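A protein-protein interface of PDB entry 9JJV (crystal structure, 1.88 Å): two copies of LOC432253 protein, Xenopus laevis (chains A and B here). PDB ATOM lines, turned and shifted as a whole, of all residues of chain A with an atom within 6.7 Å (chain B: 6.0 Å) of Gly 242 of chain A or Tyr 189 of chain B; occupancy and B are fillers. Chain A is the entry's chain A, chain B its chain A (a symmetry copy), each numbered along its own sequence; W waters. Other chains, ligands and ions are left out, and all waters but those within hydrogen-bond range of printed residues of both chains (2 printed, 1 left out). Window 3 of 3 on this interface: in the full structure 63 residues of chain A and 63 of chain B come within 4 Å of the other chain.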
ATOM      1  N   TRP A  86      -9.150   2.479 -21.211  1.00  0.00           N
ATOM      2  CA  TRP A  86      -9.990   3.472 -21.874  1.00  0.00           C
ATOM      3  C   TRP A  86     -11.416   2.918 -21.937  1.00  0.00           C
ATOM      4  O   TRP A  86     -11.616   1.708 -22.038  1.00  0.00           O
ATOM      5  CB  TRP A  86      -9.434   3.807 -23.282  1.00  0.00           C
ATOM      6  CG  TRP A  86      -9.531   2.635 -24.255  1.00  0.00           C
ATOM      7  CD1 TRP A  86      -8.672   1.579 -24.359  1.00  0.00           C
ATOM      8  CD2 TRP A  86     -10.564   2.406 -25.222  1.00  0.00           C
ATOM      9  NE1 TRP A  86      -9.105   0.709 -25.338  1.00  0.00           N
ATOM     10  CE2 TRP A  86     -10.262   1.196 -25.882  1.00  0.00           C
ATOM     11  CE3 TRP A  86     -11.718   3.111 -25.596  1.00  0.00           C
ATOM     12  CZ2 TRP A  86     -11.066   0.678 -26.897  1.00  0.00           C
ATOM     13  CZ3 TRP A  86     -12.516   2.596 -26.599  1.00  0.00           C
ATOM     14  CH2 TRP A  86     -12.193   1.390 -27.235  1.00  0.00           C
ATOM     15  N   PRO A  88     -15.933   3.859 -22.664  1.00  0.00           N
ATOM     16  CA  PRO A  88     -16.941   4.815 -23.138  1.00  0.00           C
ATOM     17  C   PRO A  88     -17.845   5.312 -22.018  1.00  0.00           C
ATOM     18  O   PRO A  88     -17.931   4.739 -20.935  1.00  0.00           O
ATOM     19  CB  PRO A  88     -17.747   4.001 -24.150  1.00  0.00           C
ATOM     20  CG  PRO A  88     -17.706   2.607 -23.584  1.00  0.00           C
ATOM     21  CD  PRO A  88     -16.293   2.468 -23.006  1.00  0.00           C
ATOM     22  N   GLY A  89     -18.547   6.396 -22.308  1.00  0.00           N
ATOM     23  CA  GLY A  89     -19.598   6.844 -21.428  1.00  0.00           C
ATOM     24  C   GLY A  89     -19.150   7.950 -20.497  1.00  0.00           C
ATOM     25  O   GLY A  89     -18.082   8.559 -20.634  1.00  0.00           O
ATOM     26  N   THR A  90     -19.992   8.184 -19.505  1.00  0.00           N
ATOM     27  CA  THR A  90     -19.842   9.335 -18.638  1.00  0.00           C
ATOM     28  C   THR A  90     -19.026   9.056 -17.382  1.00  0.00           C
ATOM     29  O   THR A  90     -18.674  10.007 -16.680  1.00  0.00           O
ATOM     30  CB  THR A  90     -21.219   9.867 -18.236  1.00  0.00           C
ATOM     31  OG1 THR A  90     -21.903   8.890 -17.443  1.00  0.00           O
ATOM     32  CG2 THR A  90     -22.037  10.181 -19.478  1.00  0.00           C
ATOM     33  N   GLY A 237     -16.888   9.785 -34.767  1.00  0.00           N
ATOM     34  CA  GLY A 237     -18.107   9.146 -35.204  1.00  0.00           C
ATOM     35  C   GLY A 237     -18.623   8.155 -34.182  1.00  0.00           C
ATOM     36  O   GLY A 237     -17.938   7.779 -33.223  1.00  0.00           O
ATOM     37  N   LYS A 238     -19.862   7.711 -34.403  1.00  0.00           N
ATOM     38  CA  LYS A 238     -20.536   6.937 -33.369  1.00  0.00           C
ATOM     39  C   LYS A 238     -19.989   5.523 -33.220  1.00  0.00           C
ATOM     40  O   LYS A 238     -20.312   4.869 -32.222  1.00  0.00           O
ATOM     41  CB  LYS A 238     -22.042   6.905 -33.639  1.00  0.00           C
ATOM     42  CG  LYS A 238     -22.439   6.430 -35.002  1.00  0.00           C
ATOM     43  CD  LYS A 238     -23.861   6.942 -35.268  1.00  0.00           C
ATOM     44  CE  LYS A 238     -24.516   6.241 -36.411  1.00  0.00           C
ATOM     45  NZ  LYS A 238     -25.811   6.903 -36.756  1.00  0.00           N
ATOM     46  N   GLY A 239     -19.200   5.033 -34.178  1.00  0.00           N
ATOM     47  CA  GLY A 239     -18.520   3.747 -34.041  1.00  0.00           C
ATOM     48  C   GLY A 239     -17.333   3.772 -33.093  1.00  0.00           C
ATOM     49  O   GLY A 239     -16.761   2.713 -32.796  1.00  0.00           O
ATOM     50  N   ILE A 240     -16.929   4.959 -32.656  1.00  0.00           N
ATOM     51  CA  ILE A 240     -15.888   5.096 -31.655  1.00  0.00           C
ATOM     52  C   ILE A 240     -16.438   5.569 -30.311  1.00  0.00           C
ATOM     53  O   ILE A 240     -15.895   5.184 -29.263  1.00  0.00           O
ATOM     54  CB  ILE A 240     -14.778   6.038 -32.166  1.00  0.00           C
ATOM     55  CG1 ILE A 240     -13.992   5.364 -33.294  1.00  0.00           C
ATOM     56  CG2 ILE A 240     -13.840   6.486 -31.035  1.00  0.00           C
ATOM     57  CD1 ILE A 240     -13.057   4.233 -32.818  1.00  0.00           C
ATOM     58  N   THR A 241     -17.517   6.368 -30.290  1.00  0.00           N
ATOM     59  CA  THR A 241     -17.953   6.913 -28.998  1.00  0.00           C
ATOM     60  C   THR A 241     -18.891   5.994 -28.240  1.00  0.00           C
ATOM     61  O   THR A 241     -19.032   6.151 -27.018  1.00  0.00           O
ATOM     62  CB  THR A 241     -18.624   8.285 -29.146  1.00  0.00           C
ATOM     63  OG1 THR A 241     -19.864   8.159 -29.852  1.00  0.00           O
ATOM     64  CG2 THR A 241     -17.712   9.258 -29.853  1.00  0.00           C
ATOM     65  N   GLY A 242     -19.524   5.047 -28.913  1.00  0.00           N
ATOM     66  CA  GLY A 242     -20.385   4.084 -28.257  1.00  0.00           C
ATOM     67  C   GLY A 242     -19.616   2.853 -27.844  1.00  0.00           C
ATOM     68  O   GLY A 242     -18.397   2.883 -27.670  1.00  0.00           O
ATOM     69  N   GLU A 243     -20.333   1.747 -27.691  1.00  0.00           N
ATOM     70  CA  GLU A 243     -19.667   0.479 -27.438  1.00  0.00           C
ATOM     71  C   GLU A 243     -18.761   0.157 -28.623  1.00  0.00           C
ATOM     72  O   GLU A 243     -19.228  -0.001 -29.755  1.00  0.00           O
ATOM     73  CB  GLU A 243     -20.699  -0.621 -27.208  1.00  0.00           C
ATOM     74  CG  GLU A 243     -21.308  -0.620 -25.791  1.00  0.00           C
ATOM     75  CD  GLU A 243     -20.474   0.140 -24.744  1.00  0.00           C
ATOM     76  OE1 GLU A 243     -20.945   1.204 -24.252  1.00  0.00           O
ATOM     77  OE2 GLU A 243     -19.364  -0.329 -24.387  1.00  0.00           O
ATOM     78  N   SER A 244     -17.462   0.081 -28.368  1.00  0.00           N
ATOM     79  CA  SER A 244     -16.488   0.056 -29.442  1.00  0.00           C
ATOM     80  C   SER A 244     -15.300  -0.788 -29.016  1.00  0.00           C
ATOM     81  O   SER A 244     -14.919  -0.808 -27.843  1.00  0.00           O
ATOM     82  CB  SER A 244     -16.036   1.489 -29.779  1.00  0.00           C
ATOM     83  OG  SER A 244     -15.180   1.547 -30.903  1.00  0.00           O
ATOM     84  N   GLU A 245     -14.702  -1.464 -29.982  1.00  0.00           N
ATOM     85  CA  GLU A 245     -13.393  -2.052 -29.755  1.00  0.00           C
ATOM     86  C   GLU A 245     -12.273  -1.065 -30.034  1.00  0.00           C
ATOM     87  O   GLU A 245     -11.102  -1.397 -29.820  1.00  0.00           O
ATOM     88  CB  GLU A 245     -13.213  -3.284 -30.635  1.00  0.00           C
ATOM     89  CG  GLU A 245     -13.954  -4.495 -30.136  1.00  0.00           C
ATOM     90  CD  GLU A 245     -13.764  -5.671 -31.057  1.00  0.00           C
ATOM     91  OE1 GLU A 245     -12.856  -6.479 -30.777  1.00  0.00           O
ATOM     92  OE2 GLU A 245     -14.491  -5.766 -32.077  1.00  0.00           O
ATOM     93  N   SER B 153     -22.072  17.367 -24.324  1.00  0.00           N
ATOM     94  CA  SER B 153     -21.545  16.023 -24.072  1.00  0.00           C
ATOM     95  C   SER B 153     -22.033  15.394 -22.776  1.00  0.00           C
ATOM     96  O   SER B 153     -22.489  14.249 -22.776  1.00  0.00           O
ATOM     97  CB  SER B 153     -20.005  16.020 -24.076  1.00  0.00           C
ATOM     98  OG  SER B 153     -19.479  16.728 -25.183  1.00  0.00           O
ATOM     99  N   ASP B 187     -24.699  16.014 -28.276  1.00  0.00           N
ATOM    100  CA  ASP B 187     -23.537  15.169 -28.617  1.00  0.00           C
ATOM    101  C   ASP B 187     -23.332  14.039 -27.611  1.00  0.00           C
ATOM    102  O   ASP B 187     -22.194  13.671 -27.284  1.00  0.00           O
ATOM    103  CB  ASP B 187     -22.266  16.014 -28.734  1.00  0.00           C
ATOM    104  CG  ASP B 187     -22.428  17.142 -29.721  1.00  0.00           C
ATOM    105  OD1 ASP B 187     -23.415  17.092 -30.488  1.00  0.00           O
ATOM    106  OD2 ASP B 187     -21.594  18.078 -29.710  1.00  0.00           O
ATOM    107  N   TRP B 188     -24.441  13.495 -27.118  1.00  0.00           N
ATOM    108  CA  TRP B 188     -24.406  12.334 -26.231  1.00  0.00           C
ATOM    109  C   TRP B 188     -23.645  11.175 -26.871  1.00  0.00           C
ATOM    110  O   TRP B 188     -23.858  10.854 -28.045  1.00  0.00           O
ATOM    111  CB  TRP B 188     -25.842  11.916 -25.917  1.00  0.00           C
ATOM    112  CG  TRP B 188     -26.001  10.776 -24.986  1.00  0.00           C
ATOM    113  CD1 TRP B 188     -26.521   9.540 -25.285  1.00  0.00           C
ATOM    114  CD2 TRP B 188     -25.698  10.756 -23.587  1.00  0.00           C
ATOM    115  NE1 TRP B 188     -26.536   8.761 -24.157  1.00  0.00           N
ATOM    116  CE2 TRP B 188     -26.040   9.483 -23.106  1.00  0.00           C
ATOM    117  CE3 TRP B 188     -25.157  11.693 -22.695  1.00  0.00           C
ATOM    118  CZ2 TRP B 188     -25.860   9.122 -21.779  1.00  0.00           C
ATOM    119  CZ3 TRP B 188     -25.002  11.334 -21.377  1.00  0.00           C
ATOM    120  CH2 TRP B 188     -25.337  10.055 -20.933  1.00  0.00           C
ATOM    121  N   TYR B 189     -22.787  10.513 -26.073  1.00  0.00           N
ATOM    122  CA  TYR B 189     -21.832   9.537 -26.613  1.00  0.00           C
ATOM    123  C   TYR B 189     -22.502   8.352 -27.298  1.00  0.00           C
ATOM    124  O   TYR B 189     -21.924   7.777 -28.224  1.00  0.00           O
ATOM    125  CB  TYR B 189     -20.899   9.011 -25.509  1.00  0.00           C
ATOM    126  CG  TYR B 189     -21.542   7.994 -24.584  1.00  0.00           C
ATOM    127  CD1 TYR B 189     -22.324   8.415 -23.504  1.00  0.00           C
ATOM    128  CD2 TYR B 189     -21.369   6.622 -24.771  1.00  0.00           C
ATOM    129  CE1 TYR B 189     -22.922   7.504 -22.648  1.00  0.00           C
ATOM    130  CE2 TYR B 189     -21.974   5.699 -23.917  1.00  0.00           C
ATOM    131  CZ  TYR B 189     -22.751   6.151 -22.862  1.00  0.00           C
ATOM    132  OH  TYR B 189     -23.346   5.264 -21.997  1.00  0.00           O
ATOM    133  N   HIS B 190     -23.689   7.950 -26.853  1.00  0.00           N
ATOM    134  CA  HIS B 190     -24.332   6.728 -27.354  1.00  0.00           C
ATOM    135  C   HIS B 190     -25.442   7.077 -28.344  1.00  0.00           C
ATOM    136  O   HIS B 190     -26.480   7.621 -27.967  1.00  0.00           O
ATOM    137  CB  HIS B 190     -24.860   5.883 -26.200  1.00  0.00           C
ATOM    138  CG  HIS B 190     -24.885   4.413 -26.494  1.00  0.00           C
ATOM    139  ND1 HIS B 190     -25.507   3.893 -27.608  1.00  0.00           N
ATOM    140  CD2 HIS B 190     -24.356   3.358 -25.830  1.00  0.00           C
ATOM    141  CE1 HIS B 190     -25.368   2.577 -27.615  1.00  0.00           C
ATOM    142  NE2 HIS B 190     -24.670   2.227 -26.549  1.00  0.00           N
ATOM    143  N   SER B 191     -25.227   6.744 -29.613  1.00  0.00           N
ATOM    144  CA  SER B 191     -26.206   7.056 -30.639  1.00  0.00           C
ATOM    145  C   SER B 191     -27.448   6.179 -30.556  1.00  0.00           C
ATOM    146  O   SER B 191     -28.458   6.520 -31.176  1.00  0.00           O
ATOM    147  CB  SER B 191     -25.572   6.915 -32.028  1.00  0.00           C
ATOM    148  OG  SER B 191     -24.807   8.074 -32.333  1.00  0.00           O
ATOM    149  N   LYS B 193     -28.593   4.546 -27.292  1.00  0.00           N
ATOM    150  CA  LYS B 193     -29.170   4.486 -25.954  1.00  0.00           C
ATOM    151  C   LYS B 193     -29.225   5.910 -25.403  1.00  0.00           C
ATOM    152  O   LYS B 193     -28.289   6.382 -24.762  1.00  0.00           O
ATOM    153  CB  LYS B 193     -28.374   3.531 -25.062  1.00  0.00           C
ATOM    154  CG  LYS B 193     -28.531   2.070 -25.479  1.00  0.00           C
ATOM    155  CD  LYS B 193     -27.482   1.192 -24.827  1.00  0.00           C
ATOM    156  CE  LYS B 193     -27.509  -0.216 -25.390  1.00  0.00           C
ATOM    157  NZ  LYS B 193     -26.585  -1.080 -24.627  1.00  0.00           N
ATOM    158  N   LEU B 233     -29.467  14.024 -26.714  1.00  0.00           N
ATOM    159  CA  LEU B 233     -29.435  13.997 -28.183  1.00  0.00           C
ATOM    160  C   LEU B 233     -28.087  13.454 -28.632  1.00  0.00           C
ATOM    161  O   LEU B 233     -27.053  14.017 -28.246  1.00  0.00           O
ATOM    162  CB  LEU B 233     -29.643  15.393 -28.783  1.00  0.00           C
ATOM    163  CG  LEU B 233     -30.859  16.213 -28.357  1.00  0.00           C
ATOM    164  CD1 LEU B 233     -31.026  17.431 -29.268  1.00  0.00           C
ATOM    165  CD2 LEU B 233     -32.112  15.364 -28.348  1.00  0.00           C
ATOM    166  N   PRO B 234     -28.015  12.400 -29.445  1.00  0.00           N
ATOM    167  CA  PRO B 234     -26.715  11.994 -30.000  1.00  0.00           C
ATOM    168  C   PRO B 234     -26.143  13.085 -30.900  1.00  0.00           C
ATOM    169  O   PRO B 234     -26.781  14.098 -31.194  1.00  0.00           O
ATOM    170  CB  PRO B 234     -27.032  10.705 -30.778  1.00  0.00           C
ATOM    171  CG  PRO B 234     -28.501  10.583 -30.818  1.00  0.00           C
ATOM    172  CD  PRO B 234     -29.062  11.393 -29.682  1.00  0.00           C
HETATM  173  O   HOH W   1     -22.654   5.830 -30.323  1.00  0.00           O
HETATM  174  O   HOH W   2     -22.269   6.154 -19.541  1.00  0.00           O
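NE1 of Trp 188 of chain B is in hydrogen-bond range of O of Lys 193 of chain B, 3.0 Å away. N of Trp 188 of chain B sits at hydrogen-bond distance from O of Leu 233 of chain B, 2.9 Å away.
Of chain B, only Tyr 189 comes within 4 Å of Gly 242 of chain A. Of chain A, only Gly 89 (3.5 Å), Thr 241 (2.7 Å) and Gly 242 (3.7 Å) come within 4 Å of Tyr 189 of chain B. Of the printed residues of chain B, Lys 238 of chain A touches Ser 191. Printed residues of chain B within 4 Å of Thr 90 of chain A: Trp 188 (3.6 Å). Trp 86 of chain A touches none of the printed residues of chain B. Leu 233 of chain B touches none of the printed residues of chain A. The nearest residue of chain B that does not touch Gly 242 of chain A is His 190 of chain B (4.7 Å). The nearest printed residue of chain B that does not touch Thr 241 of chain A is His 190 of chain B (4.9 Å).
Printed residues of chain B that touch a printed residue of chain A: Trp 188, Tyr 189 and Ser 191.
Among the printed residues, merely in contact across the chains: Lys 238 of chain A with Ser 191 of chain B (3.3 Å), Gly 89 of chain A with Tyr 189 of chain B (3.5 Å), Thr 90 of chain A with Trp 188 of chain B (3.6 Å) and Gly 242 of chain A with Tyr 189 of chain B (3.7 Å).
OG1 of Thr 241 of chain A lies within hydrogen-bond range of O of Tyr 189 of chain B.
No position is printed for both chains.
Water W1 lies within hydrogen-bond range of N of Ser 191 of chain B (2.8 Å), O of Tyr 189 of chain B (3.0 Å) and O of Lys 238 of chain A (3.2 Å). Water W2 lies within hydrogen-bond range of OH of Tyr 189 of chain B and N of Thr 90 of chain A.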
